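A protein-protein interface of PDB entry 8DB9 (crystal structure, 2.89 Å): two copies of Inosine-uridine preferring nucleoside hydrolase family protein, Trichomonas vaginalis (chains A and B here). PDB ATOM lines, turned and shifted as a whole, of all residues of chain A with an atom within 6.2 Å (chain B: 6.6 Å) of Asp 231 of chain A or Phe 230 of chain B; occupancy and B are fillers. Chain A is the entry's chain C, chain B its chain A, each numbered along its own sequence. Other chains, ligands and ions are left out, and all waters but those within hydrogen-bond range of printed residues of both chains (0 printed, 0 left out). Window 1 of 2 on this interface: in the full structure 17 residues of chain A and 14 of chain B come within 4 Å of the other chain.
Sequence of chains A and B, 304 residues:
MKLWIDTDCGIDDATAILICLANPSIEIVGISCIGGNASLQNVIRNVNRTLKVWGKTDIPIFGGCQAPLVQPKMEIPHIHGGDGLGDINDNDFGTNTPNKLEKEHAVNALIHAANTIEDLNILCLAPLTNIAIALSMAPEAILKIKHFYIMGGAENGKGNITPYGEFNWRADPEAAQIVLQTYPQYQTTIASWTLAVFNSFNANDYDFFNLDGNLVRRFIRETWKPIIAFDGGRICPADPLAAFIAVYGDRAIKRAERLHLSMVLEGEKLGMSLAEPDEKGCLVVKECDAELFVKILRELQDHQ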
ATOM      1  N   ILE A 161      15.841   0.388 -20.208  1.00  0.00           N
ATOM      2  CA  ILE A 161      15.241  -0.330 -21.332  1.00  0.00           C
ATOM      3  C   ILE A 161      14.968  -1.779 -20.941  1.00  0.00           C
ATOM      4  O   ILE A 161      15.819  -2.450 -20.339  1.00  0.00           O
ATOM      5  CB  ILE A 161      16.179  -0.277 -22.550  1.00  0.00           C
ATOM      6  CG1 ILE A 161      16.776   1.109 -22.715  1.00  0.00           C
ATOM      7  CG2 ILE A 161      15.457  -0.684 -23.848  1.00  0.00           C
ATOM      8  CD1 ILE A 161      15.831   2.099 -23.328  1.00  0.00           C
ATOM      9  N   TRP A 193      19.154  -4.118 -29.033  1.00  0.00           N
ATOM     10  CA  TRP A 193      17.865  -3.452 -29.114  1.00  0.00           C
ATOM     11  C   TRP A 193      17.846  -2.246 -28.212  1.00  0.00           C
ATOM     12  O   TRP A 193      17.222  -1.235 -28.531  1.00  0.00           O
ATOM     13  CB  TRP A 193      16.750  -4.422 -28.752  1.00  0.00           C
ATOM     14  CG  TRP A 193      15.441  -3.802 -28.392  1.00  0.00           C
ATOM     15  CD1 TRP A 193      14.788  -3.917 -27.203  1.00  0.00           C
ATOM     16  CD2 TRP A 193      14.604  -3.008 -29.232  1.00  0.00           C
ATOM     17  NE1 TRP A 193      13.599  -3.242 -27.243  1.00  0.00           N
ATOM     18  CE2 TRP A 193      13.457  -2.674 -28.481  1.00  0.00           C
ATOM     19  CE3 TRP A 193      14.706  -2.544 -30.551  1.00  0.00           C
ATOM     20  CZ2 TRP A 193      12.421  -1.902 -29.003  1.00  0.00           C
ATOM     21  CZ3 TRP A 193      13.679  -1.769 -31.062  1.00  0.00           C
ATOM     22  CH2 TRP A 193      12.553  -1.457 -30.288  1.00  0.00           C
ATOM     23  N   VAL A 197      16.964   1.622 -29.253  1.00  0.00           N
ATOM     24  CA  VAL A 197      16.014   2.537 -28.640  1.00  0.00           C
ATOM     25  C   VAL A 197      16.722   3.803 -28.168  1.00  0.00           C
ATOM     26  O   VAL A 197      16.278   4.914 -28.456  1.00  0.00           O
ATOM     27  CB  VAL A 197      15.246   1.828 -27.512  1.00  0.00           C
ATOM     28  CG1 VAL A 197      14.297   2.776 -26.851  1.00  0.00           C
ATOM     29  CG2 VAL A 197      14.452   0.683 -28.085  1.00  0.00           C
ATOM     30  N   SER A 200      16.707   6.422 -30.705  1.00  0.00           N
ATOM     31  CA  SER A 200      15.410   6.681 -31.300  1.00  0.00           C
ATOM     32  C   SER A 200      15.175   8.180 -31.454  1.00  0.00           C
ATOM     33  O   SER A 200      15.512   8.982 -30.575  1.00  0.00           O
ATOM     34  CB  SER A 200      14.294   6.099 -30.445  1.00  0.00           C
ATOM     35  OG  SER A 200      13.750   7.138 -29.656  1.00  0.00           O
ATOM     36  N   PRO A 226       3.890   2.290 -40.286  1.00  0.00           N
ATOM     37  CA  PRO A 226       3.338   1.318 -39.319  1.00  0.00           C
ATOM     38  C   PRO A 226       4.230   1.051 -38.131  1.00  0.00           C
ATOM     39  O   PRO A 226       3.730   0.871 -37.014  1.00  0.00           O
ATOM     40  CB  PRO A 226       3.185   0.046 -40.157  1.00  0.00           C
ATOM     41  CG  PRO A 226       3.203   0.507 -41.550  1.00  0.00           C
ATOM     42  CD  PRO A 226       4.116   1.661 -41.596  1.00  0.00           C
ATOM     43  N   ILE A 227       5.543   0.995 -38.346  1.00  0.00           N
ATOM     44  CA  ILE A 227       6.453   0.709 -37.250  1.00  0.00           C
ATOM     45  C   ILE A 227       6.564   1.900 -36.320  1.00  0.00           C
ATOM     46  O   ILE A 227       6.645   1.741 -35.105  1.00  0.00           O
ATOM     47  CB  ILE A 227       7.819   0.268 -37.794  1.00  0.00           C
ATOM     48  CG1 ILE A 227       7.723  -1.196 -38.174  1.00  0.00           C
ATOM     49  CG2 ILE A 227       8.891   0.435 -36.754  1.00  0.00           C
ATOM     50  CD1 ILE A 227       7.149  -2.027 -37.044  1.00  0.00           C
ATOM     51  N   ILE A 228       6.546   3.108 -36.863  1.00  0.00           N
ATOM     52  CA  ILE A 228       6.533   4.264 -35.987  1.00  0.00           C
ATOM     53  C   ILE A 228       5.265   4.273 -35.134  1.00  0.00           C
ATOM     54  O   ILE A 228       5.331   4.393 -33.899  1.00  0.00           O
ATOM     55  CB  ILE A 228       6.719   5.551 -36.811  1.00  0.00           C
ATOM     56  CG1 ILE A 228       7.964   5.404 -37.702  1.00  0.00           C
ATOM     57  CG2 ILE A 228       6.880   6.746 -35.895  1.00  0.00           C
ATOM     58  CD1 ILE A 228       8.312   6.612 -38.536  1.00  0.00           C
ATOM     59  N   ALA A 229       4.087   4.152 -35.767  1.00  0.00           N
ATOM     60  CA  ALA A 229       2.849   4.220 -34.987  1.00  0.00           C
ATOM     61  C   ALA A 229       2.798   3.097 -33.962  1.00  0.00           C
ATOM     62  O   ALA A 229       2.391   3.306 -32.806  1.00  0.00           O
ATOM     63  CB  ALA A 229       1.626   4.162 -35.899  1.00  0.00           C
ATOM     64  N   PHE A 230       3.248   1.903 -34.361  1.00  0.00           N
ATOM     65  CA  PHE A 230       3.372   0.775 -33.457  1.00  0.00           C
ATOM     66  C   PHE A 230       4.390   1.015 -32.350  1.00  0.00           C
ATOM     67  O   PHE A 230       4.165   0.576 -31.223  1.00  0.00           O
ATOM     68  CB  PHE A 230       3.746  -0.465 -34.268  1.00  0.00           C
ATOM     69  CG  PHE A 230       4.107  -1.657 -33.432  1.00  0.00           C
ATOM     70  CD1 PHE A 230       3.175  -2.669 -33.229  1.00  0.00           C
ATOM     71  CD2 PHE A 230       5.385  -1.795 -32.888  1.00  0.00           C
ATOM     72  CE1 PHE A 230       3.487  -3.774 -32.471  1.00  0.00           C
ATOM     73  CE2 PHE A 230       5.712  -2.882 -32.112  1.00  0.00           C
ATOM     74  CZ  PHE A 230       4.758  -3.879 -31.898  1.00  0.00           C
ATOM     75  N   ASP A 231       5.506   1.683 -32.648  1.00  0.00           N
ATOM     76  CA  ASP A 231       6.589   1.970 -31.713  1.00  0.00           C
ATOM     77  C   ASP A 231       6.315   3.221 -30.892  1.00  0.00           C
ATOM     78  O   ASP A 231       7.233   3.774 -30.276  1.00  0.00           O
ATOM     79  CB  ASP A 231       7.910   2.139 -32.471  1.00  0.00           C
ATOM     80  CG  ASP A 231       8.821   0.904 -32.385  1.00  0.00           C
ATOM     81  OD1 ASP A 231       8.363  -0.161 -31.898  1.00  0.00           O
ATOM     82  OD2 ASP A 231      10.014   1.007 -32.789  1.00  0.00           O
ATOM     83  N   GLY A 232       5.101   3.740 -30.976  1.00  0.00           N
ATOM     84  CA  GLY A 232       4.735   4.845 -30.119  1.00  0.00           C
ATOM     85  C   GLY A 232       5.190   6.164 -30.678  1.00  0.00           C
ATOM     86  O   GLY A 232       5.597   7.060 -29.924  1.00  0.00           O
ATOM     87  N   GLY A 233       5.170   6.294 -31.996  1.00  0.00           N
ATOM     88  CA  GLY A 233       5.663   7.505 -32.607  1.00  0.00           C
ATOM     89  C   GLY A 233       7.164   7.685 -32.545  1.00  0.00           C
ATOM     90  O   GLY A 233       7.634   8.826 -32.575  1.00  0.00           O
ATOM     91  N   ARG A 234       7.940   6.590 -32.466  1.00  0.00           N
ATOM     92  CA  ARG A 234       9.397   6.686 -32.427  1.00  0.00           C
ATOM     93  C   ARG A 234      10.061   5.808 -33.488  1.00  0.00           C
ATOM     94  O   ARG A 234       9.630   4.680 -33.753  1.00  0.00           O
ATOM     95  CB  ARG A 234       9.955   6.316 -31.041  1.00  0.00           C
ATOM     96  CG  ARG A 234       9.426   7.185 -29.919  1.00  0.00           C
ATOM     97  CD  ARG A 234      10.336   7.154 -28.691  1.00  0.00           C
ATOM     98  NE  ARG A 234      11.504   8.041 -28.821  1.00  0.00           N
ATOM     99  CZ  ARG A 234      11.601   9.271 -28.309  1.00  0.00           C
ATOM    100  NH1 ARG A 234      10.593   9.792 -27.613  1.00  0.00           N
ATOM    101  NH2 ARG A 234      12.714   9.977 -28.491  1.00  0.00           N
ATOM    102  N   ILE A 235      11.148   6.347 -34.054  1.00  0.00           N
ATOM    103  CA  ILE A 235      12.002   5.686 -35.042  1.00  0.00           C
ATOM    104  C   ILE A 235      13.147   4.996 -34.305  1.00  0.00           C
ATOM    105  O   ILE A 235      14.088   5.668 -33.875  1.00  0.00           O
ATOM    106  CB  ILE A 235      12.568   6.694 -36.057  1.00  0.00           C
ATOM    107  CG1 ILE A 235      11.452   7.487 -36.748  1.00  0.00           C
ATOM    108  CG2 ILE A 235      13.478   5.998 -37.071  1.00  0.00           C
ATOM    109  CD1 ILE A 235      11.935   8.745 -37.381  1.00  0.00           C
ATOM    110  N   CYS A 236      13.098   3.663 -34.173  1.00  0.00           N
ATOM    111  CA  CYS A 236      14.144   2.847 -33.544  1.00  0.00           C
ATOM    112  C   CYS A 236      14.907   2.053 -34.597  1.00  0.00           C
ATOM    113  O   CYS A 236      14.579   0.887 -34.859  1.00  0.00           O
ATOM    114  CB  CYS A 236      13.531   1.896 -32.522  1.00  0.00           C
ATOM    115  SG  CYS A 236      12.515   2.630 -31.251  1.00  0.00           S
ATOM    116  N   ILE B  76       2.507  -4.567 -26.417  1.00  0.00           N
ATOM    117  CA  ILE B  76       3.735  -3.778 -26.544  1.00  0.00           C
ATOM    118  C   ILE B  76       4.736  -4.066 -25.421  1.00  0.00           C
ATOM    119  O   ILE B  76       4.964  -3.201 -24.557  1.00  0.00           O
ATOM    120  CB  ILE B  76       3.412  -2.277 -26.621  1.00  0.00           C
ATOM    121  CG1 ILE B  76       2.321  -1.891 -25.643  1.00  0.00           C
ATOM    122  CG2 ILE B  76       2.942  -1.907 -27.996  1.00  0.00           C
ATOM    123  CD1 ILE B  76       2.198  -0.386 -25.536  1.00  0.00           C
ATOM    124  N   HIS B  78       7.855  -4.005 -25.396  1.00  0.00           N
ATOM    125  CA  HIS B  78       9.004  -3.117 -25.397  1.00  0.00           C
ATOM    126  C   HIS B  78       8.724  -1.802 -24.703  1.00  0.00           C
ATOM    127  O   HIS B  78       9.667  -1.103 -24.325  1.00  0.00           O
ATOM    128  CB  HIS B  78       9.494  -2.850 -26.819  1.00  0.00           C
ATOM    129  CG  HIS B  78       8.436  -2.379 -27.767  1.00  0.00           C
ATOM    130  ND1 HIS B  78       8.379  -1.082 -28.226  1.00  0.00           N
ATOM    131  CD2 HIS B  78       7.430  -3.043 -28.389  1.00  0.00           C
ATOM    132  CE1 HIS B  78       7.374  -0.961 -29.074  1.00  0.00           C
ATOM    133  NE2 HIS B  78       6.784  -2.136 -29.193  1.00  0.00           N
ATOM    134  N   ILE B  79       7.460  -1.449 -24.508  1.00  0.00           N
ATOM    135  CA  ILE B  79       7.115  -0.203 -23.839  1.00  0.00           C
ATOM    136  C   ILE B  79       6.682  -0.435 -22.394  1.00  0.00           C
ATOM    137  O   ILE B  79       7.072   0.322 -21.509  1.00  0.00           O
ATOM    138  CB  ILE B  79       6.039   0.560 -24.641  1.00  0.00           C
ATOM    139  CG1 ILE B  79       6.499   0.748 -26.096  1.00  0.00           C
ATOM    140  CG2 ILE B  79       5.759   1.915 -24.008  1.00  0.00           C
ATOM    141  CD1 ILE B  79       5.620   1.673 -26.925  1.00  0.00           C
ATOM    142  N   ARG B 170      -6.095   3.174 -32.155  1.00  0.00           N
ATOM    143  CA  ARG B 170      -5.474   2.484 -33.282  1.00  0.00           C
ATOM    144  C   ARG B 170      -5.534   0.967 -33.110  1.00  0.00           C
ATOM    145  O   ARG B 170      -5.353   0.232 -34.089  1.00  0.00           O
ATOM    146  CB  ARG B 170      -4.026   2.979 -33.451  1.00  0.00           C
ATOM    147  CG  ARG B 170      -3.332   2.596 -34.767  1.00  0.00           C
ATOM    148  CD  ARG B 170      -1.925   2.070 -34.531  1.00  0.00           C
ATOM    149  NE  ARG B 170      -1.185   2.973 -33.651  1.00  0.00           N
ATOM    150  CZ  ARG B 170      -0.696   2.632 -32.458  1.00  0.00           C
ATOM    151  NH1 ARG B 170      -0.870   1.397 -31.995  1.00  0.00           N
ATOM    152  NH2 ARG B 170      -0.034   3.530 -31.730  1.00  0.00           N
ATOM    153  N   LYS B 225       9.583   2.942 -14.553  1.00  0.00           N
ATOM    154  CA  LYS B 225      10.943   3.023 -15.090  1.00  0.00           C
ATOM    155  C   LYS B 225      11.024   2.802 -16.598  1.00  0.00           C
ATOM    156  O   LYS B 225      11.467   3.712 -17.318  1.00  0.00           O
ATOM    157  CB  LYS B 225      11.868   2.028 -14.366  1.00  0.00           C
ATOM    158  CG  LYS B 225      12.231   2.430 -12.929  1.00  0.00           C
ATOM    159  CD  LYS B 225      13.695   2.237 -12.614  1.00  0.00           C
ATOM    160  CE  LYS B 225      14.022   0.806 -12.171  1.00  0.00           C
ATOM    161  NZ  LYS B 225      15.309   0.714 -11.336  1.00  0.00           N
ATOM    162  N   PRO B 226      10.573   1.629 -17.125  1.00  0.00           N
ATOM    163  CA  PRO B 226      10.821   1.278 -18.543  1.00  0.00           C
ATOM    164  C   PRO B 226      10.146   2.160 -19.586  1.00  0.00           C
ATOM    165  O   PRO B 226      10.768   2.527 -20.587  1.00  0.00           O
ATOM    166  CB  PRO B 226      10.269  -0.154 -18.648  1.00  0.00           C
ATOM    167  CG  PRO B 226      10.032  -0.590 -17.267  1.00  0.00           C
ATOM    168  CD  PRO B 226       9.723   0.615 -16.487  1.00  0.00           C
ATOM    169  N   ILE B 227       8.853   2.438 -19.388  1.00  0.00           N
ATOM    170  CA  ILE B 227       8.095   3.273 -20.311  1.00  0.00           C
ATOM    171  C   ILE B 227       8.577   4.718 -20.242  1.00  0.00           C
ATOM    172  O   ILE B 227       8.599   5.418 -21.258  1.00  0.00           O
ATOM    173  CB  ILE B 227       6.582   3.128 -20.025  1.00  0.00           C
ATOM    174  CG1 ILE B 227       5.730   3.878 -21.048  1.00  0.00           C
ATOM    175  CG2 ILE B 227       6.206   3.539 -18.591  1.00  0.00           C
ATOM    176  CD1 ILE B 227       4.267   3.454 -21.031  1.00  0.00           C
ATOM    177  N   ILE B 228       8.988   5.184 -19.060  1.00  0.00           N
ATOM    178  CA  ILE B 228       9.655   6.477 -18.977  1.00  0.00           C
ATOM    179  C   ILE B 228      10.886   6.485 -19.875  1.00  0.00           C
ATOM    180  O   ILE B 228      11.023   7.344 -20.755  1.00  0.00           O
ATOM    181  CB  ILE B 228      10.011   6.816 -17.517  1.00  0.00           C
ATOM    182  CG1 ILE B 228       8.760   7.044 -16.663  1.00  0.00           C
ATOM    183  CG2 ILE B 228      10.848   8.072 -17.462  1.00  0.00           C
ATOM    184  CD1 ILE B 228       9.039   7.808 -15.346  1.00  0.00           C
ATOM    185  N   ALA B 229      11.796   5.517 -19.679  1.00  0.00           N
ATOM    186  CA  ALA B 229      13.024   5.471 -20.483  1.00  0.00           C
ATOM    187  C   ALA B 229      12.772   5.171 -21.968  1.00  0.00           C
ATOM    188  O   ALA B 229      13.683   5.362 -22.782  1.00  0.00           O
ATOM    189  CB  ALA B 229      14.003   4.442 -19.908  1.00  0.00           C
ATOM    190  N   PHE B 230      11.562   4.737 -22.308  1.00  0.00           N
ATOM    191  CA  PHE B 230      11.226   4.427 -23.694  1.00  0.00           C
ATOM    192  C   PHE B 230      10.512   5.587 -24.385  1.00  0.00           C
ATOM    193  O   PHE B 230      10.540   5.700 -25.611  1.00  0.00           O
ATOM    194  CB  PHE B 230      10.365   3.163 -23.769  1.00  0.00           C
ATOM    195  CG  PHE B 230       9.930   2.809 -25.163  1.00  0.00           C
ATOM    196  CD1 PHE B 230       8.876   3.475 -25.764  1.00  0.00           C
ATOM    197  CD2 PHE B 230      10.578   1.810 -25.872  1.00  0.00           C
ATOM    198  CE1 PHE B 230       8.474   3.151 -27.046  1.00  0.00           C
ATOM    199  CE2 PHE B 230      10.181   1.482 -27.154  1.00  0.00           C
ATOM    200  CZ  PHE B 230       9.127   2.154 -27.743  1.00  0.00           C
ATOM    201  N   ASP B 231       9.874   6.444 -23.596  1.00  0.00           N
ATOM    202  CA  ASP B 231       9.152   7.593 -24.137  1.00  0.00           C
ATOM    203  C   ASP B 231      10.076   8.788 -24.350  1.00  0.00           C
ATOM    204  O   ASP B 231       9.624   9.891 -24.656  1.00  0.00           O
ATOM    205  CB  ASP B 231       7.993   7.981 -23.216  1.00  0.00           C
ATOM    206  CG  ASP B 231       6.688   7.319 -23.612  1.00  0.00           C
ATOM    207  OD1 ASP B 231       6.669   6.605 -24.637  1.00  0.00           O
ATOM    208  OD2 ASP B 231       5.681   7.512 -22.899  1.00  0.00           O
ATOM    209  N   GLY B 232      11.374   8.557 -24.184  1.00  0.00           N
ATOM    210  CA  GLY B 232      12.372   9.591 -24.352  1.00  0.00           C
ATOM    211  C   GLY B 232      12.892  10.152 -23.057  1.00  0.00           C
ATOM    212  O   GLY B 232      13.313  11.313 -23.032  1.00  0.00           O
ATOM    213  N   GLY B 233      12.893   9.355 -21.984  1.00  0.00           N
ATOM    214  CA  GLY B 233      13.123   9.872 -20.651  1.00  0.00           C
ATOM    215  C   GLY B 233      12.009  10.764 -20.179  1.00  0.00           C
ATOM    216  O   GLY B 233      12.177  11.522 -19.218  1.00  0.00           O
ATOM    217  N   ARG B 234      10.868  10.698 -20.840  1.00  0.00           N
ATOM    218  CA  ARG B 234       9.824  11.678 -20.659  1.00  0.00           C
ATOM    219  C   ARG B 234       8.613  10.997 -20.055  1.00  0.00           C
ATOM    220  O   ARG B 234       8.299   9.851 -20.392  1.00  0.00           O
ATOM    221  CB  ARG B 234       9.480  12.355 -21.996  1.00  0.00           C
ATOM    222  CG  ARG B 234      10.314  13.626 -22.260  1.00  0.00           C
ATOM    223  CD  ARG B 234       9.637  14.579 -23.242  1.00  0.00           C
ATOM    224  NE  ARG B 234       9.665  15.993 -22.851  1.00  0.00           N
ATOM    225  CZ  ARG B 234      10.765  16.731 -22.671  1.00  0.00           C
ATOM    226  NH1 ARG B 234      11.974  16.188 -22.824  1.00  0.00           N
ATOM    227  NH2 ARG B 234      10.648  18.026 -22.339  1.00  0.00           N
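The guanidinium group of Arg 234 of chain A is in hydrogen-bond range of the backbone carbonyl oxygen of Asp 231 of chain B (3.1 Å). The backbone carbonyl oxygen of Ala 229 of chain A sits at hydrogen-bond distance from the guanidinium group of Arg 170 of chain B.
The side-chain sulfur of Cys 236 of chain A sits at hydrogen-bond distance from the side-chain carboxylate of Asp 231 of chain A (3.4 Å). OG of Ser 200 of chain A sits at hydrogen-bond distance from NE of Arg 234 of chain A, 2.6 Å away.
Among the printed residues, merely in contact across the chains: Ile 161 of chain A with Ala 229 of chain B, Trp 193 of chain A with His 78 of chain B, Val 197 of chain A with Phe 230 of chain B, Phe 230 of chain A with His 78 of chain B, Asp 231 of chain A with His 78 of chain B, Asp 231 of chain A with Phe 230 of chain B, Arg 234 of chain A with Phe 230 of chain B and Arg 234 of chain A with Gly 232 of chain B.
Printed residues of chain B within 4 Å of Ile 161 of chain A: Ala 229. Of the printed residues of chain B, Trp 193 of chain A touches His 78 (3.8 Å). Of the printed residues of chain B, Ala 229 of chain A touches Arg 170 (2.7 Å). Of chain B, only His 78 and Phe 230 come within 4 Å of Asp 231 of chain A. Printed residues of chain B within 4 Å of Arg 234 of chain A: Phe 230 (3.4 Å), Asp 231 (3.1 Å) and Gly 232 (3.7 Å). Of the printed residues of chain A, Ala 229 of chain B touches Ile 161 (3.9 Å). Phe 230 of chain B touches just these residues of chain A: Val 197 (3.97 Å), Asp 231 (3.5 Å) and Arg 234 (3.4 Å). Arg 234 of chain B touches none of the printed residues of chain A. The nearest printed residue of chain A that does not touch Ala 229 of chain B is Val 197 of chain A (4.9 Å).
Of the 15 printed residues of chain A, 7 touch a printed residue of chain B. Hydrophobic or aromatic side chains of chain A that line the printed part of chain B: Ile 161, Trp 193, Val 197, Ala 229 and Phe 230.
Asp 231 of chain A touches Phe 230 of chain B, but with the chains exchanged Phe 230 of chain A does not touch Asp 231 of chain B (9.3 Å). Arg 234 of chain A touches Phe 230 of chain B, but with the chains exchanged Phe 230 of chain A does not touch Arg 234 of chain B (14.8 Å). Arg 234 of chain A touches Asp 231 of chain B, but with the chains exchanged Asp 231 of chain A does not touch Arg 234 of chain B (11.7 Å). Arg 234 of chain A touches Gly 232 of chain B, but with the chains exchanged Gly 232 of chain A does not touch Arg 234 of chain B (10.3 Å).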
